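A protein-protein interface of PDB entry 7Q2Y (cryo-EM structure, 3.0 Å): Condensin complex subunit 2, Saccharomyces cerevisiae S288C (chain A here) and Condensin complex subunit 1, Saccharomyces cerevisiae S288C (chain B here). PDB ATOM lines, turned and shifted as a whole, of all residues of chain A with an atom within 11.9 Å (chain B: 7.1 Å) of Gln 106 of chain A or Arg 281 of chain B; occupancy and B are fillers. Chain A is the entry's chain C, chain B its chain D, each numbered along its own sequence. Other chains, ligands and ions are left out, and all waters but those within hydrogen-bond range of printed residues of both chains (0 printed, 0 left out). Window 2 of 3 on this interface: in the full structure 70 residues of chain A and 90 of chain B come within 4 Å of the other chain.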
ATOM      1  N   GLU A  96     -24.786 -33.741  33.137  1.00  0.00           N
ATOM      2  CA  GLU A  96     -23.703 -34.403  32.414  1.00  0.00           C
ATOM      3  C   GLU A  96     -23.703 -34.014  30.940  1.00  0.00           C
ATOM      4  O   GLU A  96     -22.641 -33.796  30.347  1.00  0.00           O
ATOM      5  CB  GLU A  96     -23.806 -35.918  32.573  1.00  0.00           C
ATOM      6  CG  GLU A  96     -23.487 -36.420  33.972  1.00  0.00           C
ATOM      7  CD  GLU A  96     -22.035 -36.202  34.353  1.00  0.00           C
ATOM      8  OE1 GLU A  96     -21.168 -36.253  33.456  1.00  0.00           O
ATOM      9  OE2 GLU A  96     -21.761 -35.977  35.551  1.00  0.00           O
ATOM     10  N   THR A  97     -24.889 -33.920  30.331  1.00  0.00           N
ATOM     11  CA  THR A  97     -24.973 -33.456  28.949  1.00  0.00           C
ATOM     12  C   THR A  97     -24.488 -32.015  28.826  1.00  0.00           C
ATOM     13  O   THR A  97     -23.788 -31.663  27.867  1.00  0.00           O
ATOM     14  CB  THR A  97     -26.409 -33.590  28.440  1.00  0.00           C
ATOM     15  OG1 THR A  97     -26.811 -34.965  28.501  1.00  0.00           O
ATOM     16  CG2 THR A  97     -26.519 -33.105  27.005  1.00  0.00           C
ATOM     17  N   GLY A  98     -24.857 -31.167  29.786  1.00  0.00           N
ATOM     18  CA  GLY A  98     -24.345 -29.807  29.793  1.00  0.00           C
ATOM     19  C   GLY A  98     -22.832 -29.763  29.890  1.00  0.00           C
ATOM     20  O   GLY A  98     -22.181 -28.963  29.216  1.00  0.00           O
ATOM     21  N   LYS A  99     -22.256 -30.633  30.721  1.00  0.00           N
ATOM     22  CA  LYS A  99     -20.802 -30.742  30.801  1.00  0.00           C
ATOM     23  C   LYS A  99     -20.207 -31.160  29.463  1.00  0.00           C
ATOM     24  O   LYS A  99     -19.166 -30.639  29.045  1.00  0.00           O
ATOM     25  CB  LYS A  99     -20.411 -31.743  31.888  1.00  0.00           C
ATOM     26  CG  LYS A  99     -20.166 -31.132  33.253  1.00  0.00           C
ATOM     27  CD  LYS A  99     -19.543 -32.148  34.196  1.00  0.00           C
ATOM     28  CE  LYS A  99     -20.230 -32.145  35.551  1.00  0.00           C
ATOM     29  NZ  LYS A  99     -19.583 -33.088  36.504  1.00  0.00           N
ATOM     30  N   LEU A 100     -20.848 -32.114  28.782  1.00  0.00           N
ATOM     31  CA  LEU A 100     -20.347 -32.568  27.487  1.00  0.00           C
ATOM     32  C   LEU A 100     -20.339 -31.442  26.462  1.00  0.00           C
ATOM     33  O   LEU A 100     -19.351 -31.261  25.742  1.00  0.00           O
ATOM     34  CB  LEU A 100     -21.181 -33.742  26.977  1.00  0.00           C
ATOM     35  CG  LEU A 100     -21.086 -35.025  27.797  1.00  0.00           C
ATOM     36  CD1 LEU A 100     -22.058 -36.068  27.278  1.00  0.00           C
ATOM     37  CD2 LEU A 100     -19.665 -35.539  27.742  1.00  0.00           C
ATOM     38  N   LEU A 101     -21.429 -30.676  26.377  1.00  0.00           N
ATOM     39  CA  LEU A 101     -21.449 -29.554  25.439  1.00  0.00           C
ATOM     40  C   LEU A 101     -20.481 -28.452  25.859  1.00  0.00           C
ATOM     41  O   LEU A 101     -19.913 -27.761  25.005  1.00  0.00           O
ATOM     42  CB  LEU A 101     -22.864 -28.997  25.270  1.00  0.00           C
ATOM     43  CG  LEU A 101     -23.846 -29.758  24.366  1.00  0.00           C
ATOM     44  CD1 LEU A 101     -24.333 -31.070  24.946  1.00  0.00           C
ATOM     45  CD2 LEU A 101     -25.026 -28.863  24.011  1.00  0.00           C
ATOM     46  N   SER A 102     -20.281 -28.267  27.166  1.00  0.00           N
ATOM     47  CA  SER A 102     -19.318 -27.270  27.624  1.00  0.00           C
ATOM     48  C   SER A 102     -17.898 -27.649  27.225  1.00  0.00           C
ATOM     49  O   SER A 102     -17.107 -26.790  26.819  1.00  0.00           O
ATOM     50  CB  SER A 102     -19.423 -27.095  29.139  1.00  0.00           C
ATOM     51  OG  SER A 102     -18.765 -25.914  29.562  1.00  0.00           O
ATOM     52  N   GLY A 103     -17.554 -28.935  27.337  1.00  0.00           N
ATOM     53  CA  GLY A 103     -16.218 -29.381  26.986  1.00  0.00           C
ATOM     54  C   GLY A 103     -15.975 -29.552  25.503  1.00  0.00           C
ATOM     55  O   GLY A 103     -14.819 -29.664  25.086  1.00  0.00           O
ATOM     56  N   LEU A 104     -17.037 -29.579  24.697  1.00  0.00           N
ATOM     57  CA  LEU A 104     -16.912 -29.727  23.255  1.00  0.00           C
ATOM     58  C   LEU A 104     -17.169 -28.439  22.488  1.00  0.00           C
ATOM     59  O   LEU A 104     -16.964 -28.416  21.268  1.00  0.00           O
ATOM     60  CB  LEU A 104     -17.870 -30.815  22.745  1.00  0.00           C
ATOM     61  CG  LEU A 104     -17.490 -32.263  23.063  1.00  0.00           C
ATOM     62  CD1 LEU A 104     -18.650 -33.199  22.767  1.00  0.00           C
ATOM     63  CD2 LEU A 104     -16.252 -32.675  22.283  1.00  0.00           C
ATOM     64  N   ALA A 105     -17.609 -27.372  23.158  1.00  0.00           N
ATOM     65  CA  ALA A 105     -17.885 -26.114  22.475  1.00  0.00           C
ATOM     66  C   ALA A 105     -16.622 -25.376  22.056  1.00  0.00           C
ATOM     67  O   ALA A 105     -16.707 -24.463  21.228  1.00  0.00           O
ATOM     68  CB  ALA A 105     -18.737 -25.209  23.366  1.00  0.00           C
ATOM     69  N   GLN A 106     -15.465 -25.740  22.599  1.00  0.00           N
ATOM     70  CA  GLN A 106     -14.215 -25.077  22.252  1.00  0.00           C
ATOM     71  C   GLN A 106     -13.450 -25.869  21.197  1.00  0.00           C
ATOM     72  O   GLN A 106     -12.298 -26.250  21.407  1.00  0.00           O
ATOM     73  CB  GLN A 106     -13.346 -24.880  23.496  1.00  0.00           C
ATOM     74  CG  GLN A 106     -14.044 -24.155  24.636  1.00  0.00           C
ATOM     75  CD  GLN A 106     -14.734 -25.104  25.596  1.00  0.00           C
ATOM     76  OE1 GLN A 106     -14.323 -26.255  25.752  1.00  0.00           O
ATOM     77  NE2 GLN A 106     -15.789 -24.626  26.246  1.00  0.00           N
ATOM     78  N   MET B 241      -7.380 -28.357  32.507  1.00  0.00           N
ATOM     79  CA  MET B 241      -8.616 -27.717  32.075  1.00  0.00           C
ATOM     80  C   MET B 241      -9.758 -28.722  31.989  1.00  0.00           C
ATOM     81  O   MET B 241     -10.898 -28.404  32.346  1.00  0.00           O
ATOM     82  CB  MET B 241      -8.408 -27.013  30.736  1.00  0.00           C
ATOM     83  CG  MET B 241      -9.615 -26.221  30.278  1.00  0.00           C
ATOM     84  SD  MET B 241      -9.975 -24.877  31.424  1.00  0.00           S
ATOM     85  CE  MET B 241      -8.628 -23.757  31.064  1.00  0.00           C
ATOM     86  N   THR B 242      -9.476 -29.940  31.515  1.00  0.00           N
ATOM     87  CA  THR B 242     -10.511 -30.972  31.508  1.00  0.00           C
ATOM     88  C   THR B 242     -10.969 -31.302  32.923  1.00  0.00           C
ATOM     89  O   THR B 242     -12.174 -31.420  33.183  1.00  0.00           O
ATOM     90  CB  THR B 242     -10.014 -32.234  30.799  1.00  0.00           C
ATOM     91  OG1 THR B 242      -8.876 -32.763  31.489  1.00  0.00           O
ATOM     92  CG2 THR B 242      -9.663 -31.942  29.346  1.00  0.00           C
ATOM     93  N   THR B 245     -13.185 -28.422  34.134  1.00  0.00           N
ATOM     94  CA  THR B 245     -14.505 -28.313  33.520  1.00  0.00           C
ATOM     95  C   THR B 245     -15.381 -29.514  33.858  1.00  0.00           C
ATOM     96  O   THR B 245     -16.608 -29.444  33.727  1.00  0.00           O
ATOM     97  CB  THR B 245     -14.386 -28.148  32.003  1.00  0.00           C
ATOM     98  OG1 THR B 245     -15.689 -27.948  31.443  1.00  0.00           O
ATOM     99  CG2 THR B 245     -13.778 -29.384  31.373  1.00  0.00           C
ATOM    100  N   ILE B 274      -2.886 -20.978  31.093  1.00  0.00           N
ATOM    101  CA  ILE B 274      -4.150 -21.397  31.694  1.00  0.00           C
ATOM    102  C   ILE B 274      -5.092 -20.209  31.834  1.00  0.00           C
ATOM    103  O   ILE B 274      -6.292 -20.313  31.551  1.00  0.00           O
ATOM    104  CB  ILE B 274      -3.894 -22.083  33.050  1.00  0.00           C
ATOM    105  CG1 ILE B 274      -3.319 -23.485  32.840  1.00  0.00           C
ATOM    106  CG2 ILE B 274      -5.171 -22.153  33.871  1.00  0.00           C
ATOM    107  CD1 ILE B 274      -2.835 -24.142  34.113  1.00  0.00           C
ATOM    108  N   LEU B 275      -4.567 -19.065  32.277  1.00  0.00           N
ATOM    109  CA  LEU B 275      -5.390 -17.866  32.407  1.00  0.00           C
ATOM    110  C   LEU B 275      -5.914 -17.402  31.052  1.00  0.00           C
ATOM    111  O   LEU B 275      -7.082 -17.015  30.930  1.00  0.00           O
ATOM    112  CB  LEU B 275      -4.587 -16.756  33.080  1.00  0.00           C
ATOM    113  CG  LEU B 275      -4.277 -16.989  34.557  1.00  0.00           C
ATOM    114  CD1 LEU B 275      -3.184 -16.046  35.020  1.00  0.00           C
ATOM    115  CD2 LEU B 275      -5.533 -16.824  35.398  1.00  0.00           C
ATOM    116  N   LYS B 276      -5.061 -17.431  30.025  1.00  0.00           N
ATOM    117  CA  LYS B 276      -5.509 -17.047  28.689  1.00  0.00           C
ATOM    118  C   LYS B 276      -6.609 -17.976  28.187  1.00  0.00           C
ATOM    119  O   LYS B 276      -7.607 -17.522  27.610  1.00  0.00           O
ATOM    120  CB  LYS B 276      -4.328 -17.041  27.717  1.00  0.00           C
ATOM    121  CG  LYS B 276      -3.313 -15.943  27.977  1.00  0.00           C
ATOM    122  CD  LYS B 276      -2.134 -16.046  27.022  1.00  0.00           C
ATOM    123  CE  LYS B 276      -2.538 -15.669  25.605  1.00  0.00           C
ATOM    124  NZ  LYS B 276      -2.876 -14.224  25.489  1.00  0.00           N
ATOM    125  N   GLU B 277      -6.447 -19.283  28.406  1.00  0.00           N
ATOM    126  CA  GLU B 277      -7.470 -20.233  27.983  1.00  0.00           C
ATOM    127  C   GLU B 277      -8.773 -20.014  28.743  1.00  0.00           C
ATOM    128  O   GLU B 277      -9.857 -20.083  28.155  1.00  0.00           O
ATOM    129  CB  GLU B 277      -6.970 -21.666  28.167  1.00  0.00           C
ATOM    130  CG  GLU B 277      -7.942 -22.725  27.674  1.00  0.00           C
ATOM    131  CD  GLU B 277      -7.397 -24.132  27.822  1.00  0.00           C
ATOM    132  OE1 GLU B 277      -6.266 -24.283  28.330  1.00  0.00           O
ATOM    133  OE2 GLU B 277      -8.101 -25.087  27.431  1.00  0.00           O
ATOM    134  N   ILE B 278      -8.688 -19.748  30.048  1.00  0.00           N
ATOM    135  CA  ILE B 278      -9.890 -19.480  30.834  1.00  0.00           C
ATOM    136  C   ILE B 278     -10.595 -18.236  30.313  1.00  0.00           C
ATOM    137  O   ILE B 278     -11.827 -18.199  30.205  1.00  0.00           O
ATOM    138  CB  ILE B 278      -9.533 -19.346  32.327  1.00  0.00           C
ATOM    139  CG1 ILE B 278      -9.212 -20.716  32.924  1.00  0.00           C
ATOM    140  CG2 ILE B 278     -10.664 -18.682  33.097  1.00  0.00           C
ATOM    141  CD1 ILE B 278      -8.573 -20.648  34.287  1.00  0.00           C
ATOM    142  N   SER B 279      -9.825 -17.201  29.974  1.00  0.00           N
ATOM    143  CA  SER B 279     -10.416 -15.987  29.423  1.00  0.00           C
ATOM    144  C   SER B 279     -11.105 -16.261  28.091  1.00  0.00           C
ATOM    145  O   SER B 279     -12.189 -15.727  27.825  1.00  0.00           O
ATOM    146  CB  SER B 279      -9.345 -14.910  29.262  1.00  0.00           C
ATOM    147  OG  SER B 279      -8.389 -15.284  28.285  1.00  0.00           O
ATOM    148  N   THR B 280     -10.495 -17.087  27.239  1.00  0.00           N
ATOM    149  CA  THR B 280     -11.051 -17.300  25.907  1.00  0.00           C
ATOM    150  C   THR B 280     -12.152 -18.357  25.858  1.00  0.00           C
ATOM    151  O   THR B 280     -12.856 -18.435  24.846  1.00  0.00           O
ATOM    152  CB  THR B 280      -9.943 -17.677  24.917  1.00  0.00           C
ATOM    153  OG1 THR B 280     -10.455 -17.609  23.580  1.00  0.00           O
ATOM    154  CG2 THR B 280      -9.446 -19.085  25.177  1.00  0.00           C
ATOM    155  N   ARG B 281     -12.322 -19.168  26.902  1.00  0.00           N
ATOM    156  CA  ARG B 281     -13.396 -20.159  26.892  1.00  0.00           C
ATOM    157  C   ARG B 281     -14.768 -19.506  26.991  1.00  0.00           C
ATOM    158  O   ARG B 281     -14.908 -18.365  27.443  1.00  0.00           O
ATOM    159  CB  ARG B 281     -13.236 -21.164  28.034  1.00  0.00           C
ATOM    160  CG  ARG B 281     -12.033 -22.077  27.934  1.00  0.00           C
ATOM    161  CD  ARG B 281     -11.947 -22.991  29.143  1.00  0.00           C
ATOM    162  NE  ARG B 281     -13.075 -23.911  29.220  1.00  0.00           N
ATOM    163  CZ  ARG B 281     -13.116 -25.098  28.631  1.00  0.00           C
ATOM    164  NH1 ARG B 281     -12.102 -25.546  27.907  1.00  0.00           N
ATOM    165  NH2 ARG B 281     -14.201 -25.855  28.771  1.00  0.00           N
ATOM    166  N   VAL B 282     -15.786 -20.249  26.559  1.00  0.00           N
ATOM    167  CA  VAL B 282     -17.183 -19.857  26.674  1.00  0.00           C
ATOM    168  C   VAL B 282     -17.939 -21.010  27.323  1.00  0.00           C
ATOM    169  O   VAL B 282     -17.542 -22.174  27.213  1.00  0.00           O
ATOM    170  CB  VAL B 282     -17.788 -19.490  25.298  1.00  0.00           C
ATOM    171  CG1 VAL B 282     -17.863 -20.716  24.395  1.00  0.00           C
ATOM    172  CG2 VAL B 282     -19.154 -18.828  25.451  1.00  0.00           C
ATOM    173  N   PHE B 283     -19.030 -20.681  28.012  1.00  0.00           N
ATOM    174  CA  PHE B 283     -19.792 -21.662  28.770  1.00  0.00           C
ATOM    175  C   PHE B 283     -21.249 -21.649  28.328  1.00  0.00           C
ATOM    176  O   PHE B 283     -21.750 -20.659  27.790  1.00  0.00           O
ATOM    177  CB  PHE B 283     -19.714 -21.395  30.279  1.00  0.00           C
ATOM    178  CG  PHE B 283     -18.316 -21.400  30.827  1.00  0.00           C
ATOM    179  CD1 PHE B 283     -17.695 -22.590  31.166  1.00  0.00           C
ATOM    180  CD2 PHE B 283     -17.628 -20.214  31.013  1.00  0.00           C
ATOM    181  CE1 PHE B 283     -16.410 -22.597  31.673  1.00  0.00           C
ATOM    182  CE2 PHE B 283     -16.343 -20.213  31.520  1.00  0.00           C
ATOM    183  CZ  PHE B 283     -15.733 -21.407  31.851  1.00  0.00           C
ATOM    184  N   ASN B 284     -21.922 -22.771  28.563  1.00  0.00           N
ATOM    185  CA  ASN B 284     -23.355 -22.888  28.347  1.00  0.00           C
ATOM    186  C   ASN B 284     -24.105 -22.667  29.659  1.00  0.00           C
ATOM    187  O   ASN B 284     -23.553 -22.793  30.754  1.00  0.00           O
ATOM    188  CB  ASN B 284     -23.702 -24.251  27.741  1.00  0.00           C
ATOM    189  CG  ASN B 284     -23.005 -25.397  28.442  1.00  0.00           C
ATOM    190  OD1 ASN B 284     -22.212 -25.188  29.359  1.00  0.00           O
ATOM    191  ND2 ASN B 284     -23.294 -26.620  28.012  1.00  0.00           N
ATOM    192  N   GLY B 290     -18.951 -25.930  35.369  1.00  0.00           N
ATOM    193  CA  GLY B 290     -17.701 -25.444  34.839  1.00  0.00           C
ATOM    194  C   GLY B 290     -17.401 -24.026  35.282  1.00  0.00           C
ATOM    195  O   GLY B 290     -16.293 -23.720  35.735  1.00  0.00           O
ATOM    196  N   ILE B 294     -14.327 -22.915  37.727  1.00  0.00           N
ATOM    197  CA  ILE B 294     -13.409 -21.868  37.290  1.00  0.00           C
ATOM    198  C   ILE B 294     -13.378 -20.732  38.304  1.00  0.00           C
ATOM    199  O   ILE B 294     -12.315 -20.178  38.605  1.00  0.00           O
ATOM    200  CB  ILE B 294     -13.797 -21.369  35.885  1.00  0.00           C
ATOM    201  CG1 ILE B 294     -13.486 -22.439  34.836  1.00  0.00           C
ATOM    202  CG2 ILE B 294     -13.065 -20.081  35.548  1.00  0.00           C
ATOM    203  CD1 ILE B 294     -12.017 -22.777  34.725  1.00  0.00           C
ATOM    204  N   LEU B 319     -13.845 -11.674  31.098  1.00  0.00           N
ATOM    205  CA  LEU B 319     -14.843 -12.609  31.604  1.00  0.00           C
ATOM    206  C   LEU B 319     -16.024 -11.904  32.260  1.00  0.00           C
ATOM    207  O   LEU B 319     -17.089 -12.516  32.409  1.00  0.00           O
ATOM    208  CB  LEU B 319     -14.200 -13.573  32.602  1.00  0.00           C
ATOM    209  CG  LEU B 319     -13.507 -14.804  32.016  1.00  0.00           C
ATOM    210  CD1 LEU B 319     -12.813 -15.595  33.113  1.00  0.00           C
ATOM    211  CD2 LEU B 319     -14.502 -15.678  31.268  1.00  0.00           C
ATOM    212  N   ASN B 322     -19.593 -11.821  30.657  1.00  0.00           N
ATOM    213  CA  ASN B 322     -20.472 -12.977  30.702  1.00  0.00           C
ATOM    214  C   ASN B 322     -21.564 -12.769  31.750  1.00  0.00           C
ATOM    215  O   ASN B 322     -21.426 -11.977  32.686  1.00  0.00           O
ATOM    216  CB  ASN B 322     -19.669 -14.243  31.010  1.00  0.00           C
ATOM    217  CG  ASN B 322     -20.490 -15.514  30.865  1.00  0.00           C
ATOM    218  OD1 ASN B 322     -21.682 -15.471  30.559  1.00  0.00           O
ATOM    219  ND2 ASN B 322     -19.851 -16.656  31.088  1.00  0.00           N
ATOM    220  N   LEU B 327     -18.850 -16.322  37.933  1.00  0.00           N
ATOM    221  CA  LEU B 327     -17.647 -15.831  37.266  1.00  0.00           C
ATOM    222  C   LEU B 327     -17.399 -14.360  37.573  1.00  0.00           C
ATOM    223  O   LEU B 327     -16.261 -13.960  37.843  1.00  0.00           O
ATOM    224  CB  LEU B 327     -17.750 -16.052  35.759  1.00  0.00           C
ATOM    225  CG  LEU B 327     -17.322 -17.429  35.250  1.00  0.00           C
ATOM    226  CD1 LEU B 327     -17.499 -17.523  33.743  1.00  0.00           C
ATOM    227  CD2 LEU B 327     -15.884 -17.715  35.643  1.00  0.00           C
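Of the printed residues of chain B, Leu 101 of chain A touches Asn 284. Of the printed residues of chain B, Ser 102 of chain A touches Arg 281, Phe 283 and Asn 284. Gln 106 of chain A touches just these residues of chain B: Arg 281 (3.0 Å) and Val 282 (3.2 Å). No residue of chain A comes within 4 Å of Met 241 of chain B. Leu 275 of chain B touches none of the printed residues of chain A. No residue of chain A comes within 4 Å of Glu 277 of chain B. Ile 278 of chain B touches none of the printed residues of chain A. Val 282 of chain B touches just one residue of chain A: Gln 106 (3.2 Å). Printed residues of chain A within 4 Å of Asn 284 of chain B: Gly 98, Leu 101 and Ser 102. Leu 319 of chain B touches none of the printed residues of chain A. The nearest residue of chain B that does not touch Gln 106 of chain A is Phe 283 of chain B (5.4 Å). The nearest residue of chain A that does not touch Arg 281 of chain B is Gly 103 of chain A (4.4 Å). The nearest printed residue of chain B that does not touch Lys 99 of chain A is Asn 284 of chain B (5.0 Å).
The side-chain amino group of Lys 99 of chain A is in salt-bridge range of the side-chain carboxylate of Glu 96 of chain A (3.7 Å). O of Ser 102 of chain A is in hydrogen-bond range of NE2 of Gln 106 of chain A (2.6 Å).
Thr 245 of chain B touches Lys 99 of chain A. CB of Leu 101 of chain A touches ND2 of Asn 284 of chain B (3.7 Å). NH2 of Arg 281 of chain B touches O of Ser 102 of chain A, at 3.6 Å. CD1 of Phe 283 of chain B touches OG of Ser 102 of chain A, at 3.8 Å. Ser 102 of chain A touches Asn 284 of chain B.
ND2 of Asn 284 of chain B sits at hydrogen-bond distance from O of Gly 98 of chain A (2.9 Å). OE1 of Gln 106 of chain A lies within hydrogen-bond range of NH2 of Arg 281 of chain B (3.0 Å). The backbone carbonyl oxygen (O) of Val 282 of chain B is in hydrogen-bond range of the side-chain amide nitrogen (NE2) of Gln 106 of chain A (3.2 Å).
Printed residues of chain A that touch a printed residue of chain B: Gly 98, Lys 99, Leu 101, Ser 102 and Gln 106. Hydrophobic or aromatic side chains of chain B that line the printed part of chain A: Phe 283. Along chain B the printed residues that touch a printed residue of chain A span positions 245 to 284.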
